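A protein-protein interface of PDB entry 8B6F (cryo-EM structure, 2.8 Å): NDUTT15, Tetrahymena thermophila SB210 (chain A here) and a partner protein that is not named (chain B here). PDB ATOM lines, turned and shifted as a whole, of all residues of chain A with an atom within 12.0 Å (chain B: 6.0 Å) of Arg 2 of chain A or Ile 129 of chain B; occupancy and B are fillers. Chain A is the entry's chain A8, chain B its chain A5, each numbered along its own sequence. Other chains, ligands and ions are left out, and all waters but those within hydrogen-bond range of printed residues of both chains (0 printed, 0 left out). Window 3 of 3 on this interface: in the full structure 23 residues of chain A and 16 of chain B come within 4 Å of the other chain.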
ATOM      1  N   GLN A   1       3.184  -5.099   9.880  1.00  0.00           N
ATOM      2  CA  GLN A   1       2.298  -5.528  10.998  1.00  0.00           C
ATOM      3  C   GLN A   1       3.106  -6.254  12.065  1.00  0.00           C
ATOM      4  O   GLN A   1       4.246  -6.647  11.827  1.00  0.00           O
ATOM      5  CB  GLN A   1       1.174  -6.428  10.482  1.00  0.00           C
ATOM      6  CG  GLN A   1       0.284  -5.767   9.439  1.00  0.00           C
ATOM      7  CD  GLN A   1      -0.460  -4.565   9.983  1.00  0.00           C
ATOM      8  OE1 GLN A   1      -0.602  -4.404  11.194  1.00  0.00           O
ATOM      9  NE2 GLN A   1      -0.935  -3.710   9.088  1.00  0.00           N
ATOM     10  N   ARG A   2       2.510  -6.431  13.241  1.00  0.00           N
ATOM     11  CA  ARG A   2       3.199  -7.073  14.351  1.00  0.00           C
ATOM     12  C   ARG A   2       3.206  -8.584  14.166  1.00  0.00           C
ATOM     13  O   ARG A   2       2.173  -9.187  13.861  1.00  0.00           O
ATOM     14  CB  ARG A   2       2.532  -6.708  15.677  1.00  0.00           C
ATOM     15  CG  ARG A   2       2.554  -5.219  15.985  1.00  0.00           C
ATOM     16  CD  ARG A   2       1.998  -4.936  17.371  1.00  0.00           C
ATOM     17  NE  ARG A   2       1.974  -3.508  17.667  1.00  0.00           N
ATOM     18  CZ  ARG A   2       1.601  -2.991  18.829  1.00  0.00           C
ATOM     19  NH1 ARG A   2       1.224  -3.757  19.839  1.00  0.00           N
ATOM     20  NH2 ARG A   2       1.605  -1.669  18.981  1.00  0.00           N
ATOM     21  N   GLY A   3       4.373  -9.192  14.351  1.00  0.00           N
ATOM     22  CA  GLY A   3       4.487 -10.636  14.217  1.00  0.00           C
ATOM     23  C   GLY A   3       4.057 -11.143  12.860  1.00  0.00           C
ATOM     24  O   GLY A   3       3.418 -12.199  12.767  1.00  0.00           O
ATOM     25  N   ARG A   4       4.399 -10.417  11.800  1.00  0.00           N
ATOM     26  CA  ARG A   4       3.993 -10.753  10.444  1.00  0.00           C
ATOM     27  C   ARG A   4       5.233 -10.999   9.599  1.00  0.00           C
ATOM     28  O   ARG A   4       6.183 -10.210   9.636  1.00  0.00           O
ATOM     29  CB  ARG A   4       3.148  -9.631   9.835  1.00  0.00           C
ATOM     30  CG  ARG A   4       2.540  -9.962   8.483  1.00  0.00           C
ATOM     31  CD  ARG A   4       1.506 -11.070   8.591  1.00  0.00           C
ATOM     32  NE  ARG A   4       0.754 -11.225   7.351  1.00  0.00           N
ATOM     33  CZ  ARG A   4       1.167 -11.923   6.302  1.00  0.00           C
ATOM     34  NH1 ARG A   4       2.329 -12.556   6.306  1.00  0.00           N
ATOM     35  NH2 ARG A   4       0.395 -11.987   5.222  1.00  0.00           N
ATOM     36  N   ASP A   5       5.221 -12.096   8.847  1.00  0.00           N
ATOM     37  CA  ASP A   5       6.287 -12.430   7.912  1.00  0.00           C
ATOM     38  C   ASP A   5       5.699 -12.430   6.509  1.00  0.00           C
ATOM     39  O   ASP A   5       4.756 -13.176   6.229  1.00  0.00           O
ATOM     40  CB  ASP A   5       6.902 -13.790   8.246  1.00  0.00           C
ATOM     41  CG  ASP A   5       8.146 -14.080   7.437  1.00  0.00           C
ATOM     42  OD1 ASP A   5       8.573 -13.194   6.666  1.00  0.00           O
ATOM     43  OD2 ASP A   5       8.696 -15.193   7.568  1.00  0.00           O
ATOM     44  N   TYR A   6       6.255 -11.596   5.634  1.00  0.00           N
ATOM     45  CA  TYR A   6       5.725 -11.398   4.294  1.00  0.00           C
ATOM     46  C   TYR A   6       6.376 -12.300   3.253  1.00  0.00           C
ATOM     47  O   TYR A   6       6.093 -12.148   2.061  1.00  0.00           O
ATOM     48  CB  TYR A   6       5.880  -9.933   3.881  1.00  0.00           C
ATOM     49  CG  TYR A   6       4.997  -8.992   4.665  1.00  0.00           C
ATOM     50  CD1 TYR A   6       5.418  -8.459   5.876  1.00  0.00           C
ATOM     51  CD2 TYR A   6       3.740  -8.643   4.196  1.00  0.00           C
ATOM     52  CE1 TYR A   6       4.610  -7.600   6.596  1.00  0.00           C
ATOM     53  CE2 TYR A   6       2.925  -7.785   4.906  1.00  0.00           C
ATOM     54  CZ  TYR A   6       3.365  -7.267   6.105  1.00  0.00           C
ATOM     55  OH  TYR A   6       2.554  -6.413   6.815  1.00  0.00           O
ATOM     56  N   GLU A  18      -2.559 -13.598   0.924  1.00  0.00           N
ATOM     57  CA  GLU A  18      -1.642 -13.631   2.058  1.00  0.00           C
ATOM     58  C   GLU A  18      -1.707 -12.336   2.855  1.00  0.00           C
ATOM     59  O   GLU A  18      -1.653 -12.357   4.090  1.00  0.00           O
ATOM     60  CB  GLU A  18      -0.217 -13.888   1.573  1.00  0.00           C
ATOM     61  CG  GLU A  18      -0.069 -15.166   0.767  1.00  0.00           C
ATOM     62  CD  GLU A  18       1.378 -15.501   0.474  1.00  0.00           C
ATOM     63  OE1 GLU A  18       2.264 -14.951   1.159  1.00  0.00           O
ATOM     64  OE2 GLU A  18       1.630 -16.313  -0.439  1.00  0.00           O
ATOM     65  N   LEU A  19      -1.816 -11.203   2.171  1.00  0.00           N
ATOM     66  CA  LEU A  19      -1.915  -9.917   2.838  1.00  0.00           C
ATOM     67  C   LEU A  19      -3.323  -9.700   3.380  1.00  0.00           C
ATOM     68  O   LEU A  19      -4.297 -10.296   2.914  1.00  0.00           O
ATOM     69  CB  LEU A  19      -1.556  -8.785   1.877  1.00  0.00           C
ATOM     70  CG  LEU A  19      -0.144  -8.809   1.297  1.00  0.00           C
ATOM     71  CD1 LEU A  19      -0.009  -7.752   0.220  1.00  0.00           C
ATOM     72  CD2 LEU A  19       0.890  -8.595   2.392  1.00  0.00           C
ATOM     73  N   GLU A  20      -3.421  -8.827   4.376  1.00  0.00           N
ATOM     74  CA  GLU A  20      -4.722  -8.398   4.859  1.00  0.00           C
ATOM     75  C   GLU A  20      -5.435  -7.589   3.784  1.00  0.00           C
ATOM     76  O   GLU A  20      -4.811  -6.886   2.985  1.00  0.00           O
ATOM     77  CB  GLU A  20      -4.578  -7.564   6.131  1.00  0.00           C
ATOM     78  CG  GLU A  20      -4.040  -8.347   7.315  1.00  0.00           C
ATOM     79  CD  GLU A  20      -3.964  -7.513   8.576  1.00  0.00           C
ATOM     80  OE1 GLU A  20      -4.306  -6.313   8.515  1.00  0.00           O
ATOM     81  OE2 GLU A  20      -3.562  -8.054   9.627  1.00  0.00           O
ATOM     82  N   GLU A  23      -4.653  -3.813   3.806  1.00  0.00           N
ATOM     83  CA  GLU A  23      -3.375  -3.430   3.215  1.00  0.00           C
ATOM     84  C   GLU A  23      -3.447  -3.457   1.694  1.00  0.00           C
ATOM     85  O   GLU A  23      -2.974  -2.536   1.020  1.00  0.00           O
ATOM     86  CB  GLU A  23      -2.266  -4.354   3.712  1.00  0.00           C
ATOM     87  CG  GLU A  23      -1.898  -4.148   5.164  1.00  0.00           C
ATOM     88  CD  GLU A  23      -0.699  -4.976   5.574  1.00  0.00           C
ATOM     89  OE1 GLU A  23      -0.488  -6.051   4.975  1.00  0.00           O
ATOM     90  OE2 GLU A  23       0.040  -4.547   6.485  1.00  0.00           O
ATOM     91  N   TYR A  49       7.451  -4.701   0.131  1.00  0.00           N
ATOM     92  CA  TYR A  49       7.216  -5.978   0.794  1.00  0.00           C
ATOM     93  C   TYR A  49       5.763  -6.422   0.672  1.00  0.00           C
ATOM     94  O   TYR A  49       5.476  -7.623   0.744  1.00  0.00           O
ATOM     95  CB  TYR A  49       7.631  -5.894   2.266  1.00  0.00           C
ATOM     96  CG  TYR A  49       6.870  -4.879   3.095  1.00  0.00           C
ATOM     97  CD1 TYR A  49       7.147  -3.522   2.999  1.00  0.00           C
ATOM     98  CD2 TYR A  49       5.898  -5.285   3.998  1.00  0.00           C
ATOM     99  CE1 TYR A  49       6.463  -2.596   3.762  1.00  0.00           C
ATOM    100  CE2 TYR A  49       5.207  -4.366   4.767  1.00  0.00           C
ATOM    101  CZ  TYR A  49       5.496  -3.023   4.643  1.00  0.00           C
ATOM    102  OH  TYR A  49       4.815  -2.104   5.407  1.00  0.00           O
ATOM    103  N   MET A  50       4.837  -5.482   0.488  1.00  0.00           N
ATOM    104  CA  MET A  50       3.432  -5.799   0.268  1.00  0.00           C
ATOM    105  C   MET A  50       3.043  -5.794  -1.202  1.00  0.00           C
ATOM    106  O   MET A  50       1.897  -6.119  -1.526  1.00  0.00           O
ATOM    107  CB  MET A  50       2.542  -4.807   1.020  1.00  0.00           C
ATOM    108  CG  MET A  50       2.868  -4.695   2.490  1.00  0.00           C
ATOM    109  SD  MET A  50       1.637  -3.763   3.414  1.00  0.00           S
ATOM    110  CE  MET A  50       1.681  -2.204   2.541  1.00  0.00           C
ATOM    111  N   GLN B  71      -7.459  -7.453  15.967  1.00  0.00           N
ATOM    112  CA  GLN B  71      -6.391  -7.754  16.907  1.00  0.00           C
ATOM    113  C   GLN B  71      -6.402  -6.717  18.017  1.00  0.00           C
ATOM    114  O   GLN B  71      -6.530  -5.520  17.753  1.00  0.00           O
ATOM    115  CB  GLN B  71      -5.027  -7.769  16.207  1.00  0.00           C
ATOM    116  CG  GLN B  71      -4.989  -8.672  14.982  1.00  0.00           C
ATOM    117  CD  GLN B  71      -3.655  -8.639  14.276  1.00  0.00           C
ATOM    118  OE1 GLN B  71      -2.670  -8.128  14.805  1.00  0.00           O
ATOM    119  NE2 GLN B  71      -3.614  -9.187  13.068  1.00  0.00           N
ATOM    120  N   TYR B  73      -4.686  -5.474  21.974  1.00  0.00           N
ATOM    121  CA  TYR B  73      -3.521  -5.505  22.846  1.00  0.00           C
ATOM    122  C   TYR B  73      -3.873  -4.855  24.176  1.00  0.00           C
ATOM    123  O   TYR B  73      -4.586  -3.849  24.214  1.00  0.00           O
ATOM    124  CB  TYR B  73      -2.339  -4.782  22.199  1.00  0.00           C
ATOM    125  CG  TYR B  73      -2.041  -5.265  20.800  1.00  0.00           C
ATOM    126  CD1 TYR B  73      -1.289  -6.413  20.587  1.00  0.00           C
ATOM    127  CD2 TYR B  73      -2.517  -4.578  19.693  1.00  0.00           C
ATOM    128  CE1 TYR B  73      -1.017  -6.859  19.311  1.00  0.00           C
ATOM    129  CE2 TYR B  73      -2.251  -5.016  18.411  1.00  0.00           C
ATOM    130  CZ  TYR B  73      -1.500  -6.157  18.226  1.00  0.00           C
ATOM    131  OH  TYR B  73      -1.231  -6.600  16.953  1.00  0.00           O
ATOM    132  N   HIS B  74      -3.359  -5.428  25.260  1.00  0.00           N
ATOM    133  CA  HIS B  74      -3.691  -5.009  26.614  1.00  0.00           C
ATOM    134  C   HIS B  74      -2.445  -4.489  27.316  1.00  0.00           C
ATOM    135  O   HIS B  74      -1.357  -5.051  27.168  1.00  0.00           O
ATOM    136  CB  HIS B  74      -4.300  -6.164  27.411  1.00  0.00           C
ATOM    137  CG  HIS B  74      -4.777  -5.770  28.774  1.00  0.00           C
ATOM    138  ND1 HIS B  74      -5.482  -4.610  29.007  1.00  0.00           N
ATOM    139  CD2 HIS B  74      -4.660  -6.388  29.972  1.00  0.00           C
ATOM    140  CE1 HIS B  74      -5.772  -4.525  30.294  1.00  0.00           C
ATOM    141  NE2 HIS B  74      -5.286  -5.592  30.901  1.00  0.00           N
ATOM    142  N   SER B  75      -2.613  -3.412  28.078  1.00  0.00           N
ATOM    143  CA  SER B  75      -1.546  -2.825  28.883  1.00  0.00           C
ATOM    144  C   SER B  75      -2.089  -2.585  30.283  1.00  0.00           C
ATOM    145  O   SER B  75      -2.996  -1.768  30.466  1.00  0.00           O
ATOM    146  CB  SER B  75      -1.033  -1.526  28.263  1.00  0.00           C
ATOM    147  OG  SER B  75       0.195  -1.133  28.845  1.00  0.00           O
ATOM    148  N   ASP B 127       2.460  -5.088  28.945  1.00  0.00           N
ATOM    149  CA  ASP B 127       2.491  -3.933  28.051  1.00  0.00           C
ATOM    150  C   ASP B 127       2.392  -4.366  26.592  1.00  0.00           C
ATOM    151  O   ASP B 127       3.184  -3.950  25.747  1.00  0.00           O
ATOM    152  CB  ASP B 127       3.754  -3.110  28.282  1.00  0.00           C
ATOM    153  CG  ASP B 127       3.699  -1.761  27.602  1.00  0.00           C
ATOM    154  OD1 ASP B 127       2.652  -1.440  27.004  1.00  0.00           O
ATOM    155  OD2 ASP B 127       4.699  -1.018  27.665  1.00  0.00           O
ATOM    156  N   GLU B 128       1.420  -5.223  26.274  1.00  0.00           N
ATOM    157  CA  GLU B 128       1.284  -5.671  24.893  1.00  0.00           C
ATOM    158  C   GLU B 128       1.110  -4.507  23.926  1.00  0.00           C
ATOM    159  O   GLU B 128       1.428  -4.649  22.740  1.00  0.00           O
ATOM    160  CB  GLU B 128       0.097  -6.625  24.750  1.00  0.00           C
ATOM    161  CG  GLU B 128       0.218  -7.905  25.553  1.00  0.00           C
ATOM    162  CD  GLU B 128      -1.027  -8.768  25.453  1.00  0.00           C
ATOM    163  OE1 GLU B 128      -1.991  -8.342  24.785  1.00  0.00           O
ATOM    164  OE2 GLU B 128      -1.041  -9.871  26.038  1.00  0.00           O
ATOM    165  N   ILE B 129       0.606  -3.365  24.399  1.00  0.00           N
ATOM    166  CA  ILE B 129       0.362  -2.235  23.504  1.00  0.00           C
ATOM    167  C   ILE B 129       1.665  -1.742  22.892  1.00  0.00           C
ATOM    168  O   ILE B 129       1.767  -1.554  21.674  1.00  0.00           O
ATOM    169  CB  ILE B 129      -0.375  -1.104  24.249  1.00  0.00           C
ATOM    170  CG1 ILE B 129      -1.799  -1.546  24.601  1.00  0.00           C
ATOM    171  CG2 ILE B 129      -0.357   0.184  23.433  1.00  0.00           C
ATOM    172  CD1 ILE B 129      -2.604  -0.520  25.384  1.00  0.00           C
ATOM    173  N   SER B 130       2.682  -1.522  23.726  1.00  0.00           N
ATOM    174  CA  SER B 130       3.947  -0.963  23.271  1.00  0.00           C
ATOM    175  C   SER B 130       5.175  -1.715  23.761  1.00  0.00           C
ATOM    176  O   SER B 130       6.275  -1.436  23.272  1.00  0.00           O
ATOM    177  CB  SER B 130       4.066   0.509  23.700  1.00  0.00           C
ATOM    178  OG  SER B 130       4.034   0.633  25.111  1.00  0.00           O
ATOM    179  N   ASN B 131       5.034  -2.651  24.699  1.00  0.00           N
ATOM    180  CA  ASN B 131       6.166  -3.432  25.194  1.00  0.00           C
ATOM    181  C   ASN B 131       7.277  -2.525  25.717  1.00  0.00           C
ATOM    182  O   ASN B 131       8.462  -2.762  25.479  1.00  0.00           O
ATOM    183  CB  ASN B 131       6.702  -4.366  24.108  1.00  0.00           C
ATOM    184  CG  ASN B 131       5.649  -5.330  23.599  1.00  0.00           C
ATOM    185  OD1 ASN B 131       5.215  -5.242  22.452  1.00  0.00           O
ATOM    186  ND2 ASN B 131       5.238  -6.262  24.452  1.00  0.00           N
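The backbone carbonyl oxygen (O) of Glu 128 of chain B is in hydrogen-bond range of the guanidinium group (NH1) of Arg 2 of chain A (3.0 Å). O of Ile 129 of chain B sits at hydrogen-bond distance from NH2 of Arg 2 of chain A, at 2.7 Å.
The side-chain hydroxyl (OH) of Tyr 73 of chain B is in hydrogen-bond range of the side-chain amide oxygen (OE1) of Gln 71 of chain B (3.0 Å). O of His 74 of chain B lies within hydrogen-bond range of N of Glu 128 of chain B.
CD of Arg 2 of chain A touches OH of Tyr 73 of chain B, at 3.7 Å. Gln 71 of chain B touches Glu 20 of chain A (NE2 to OE2, 3.6 Å).
Arg 2 of chain A touches three residues of chain B. Tyr 73 of chain B touches just one residue of chain A: Arg 2 (3.7 Å). No residue of chain A comes within 4 Å of Ser 75 of chain B. Asp 127 of chain B touches none of the printed residues of chain A. Of the printed residues of chain A, Glu 128 of chain B touches Arg 2 (3.0 Å). No residue of chain A comes within 4 Å of Ser 130 of chain B. Of the printed residues of chain A, Gln 71 of chain B touches Glu 20 (3.6 Å). Of the printed residues of chain B, Glu 20 of chain A touches Gln 71 (3.6 Å). The nearest residue of chain A that does not touch Ile 129 of chain B is Gln 1 of chain A (10.8 Å). The nearest printed residue of chain A that does not touch Gln 71 of chain B is Arg 2 of chain A (5.0 Å).
Of the 9 printed residues of chain B, 4 touch a printed residue of chain A. Among the printed residues, 4 pairs touch across the chains. Among the printed residues, no Asp or Glu carboxylate lies within 4 Å of a Lys or Arg side-chain nitrogen of the other chain.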
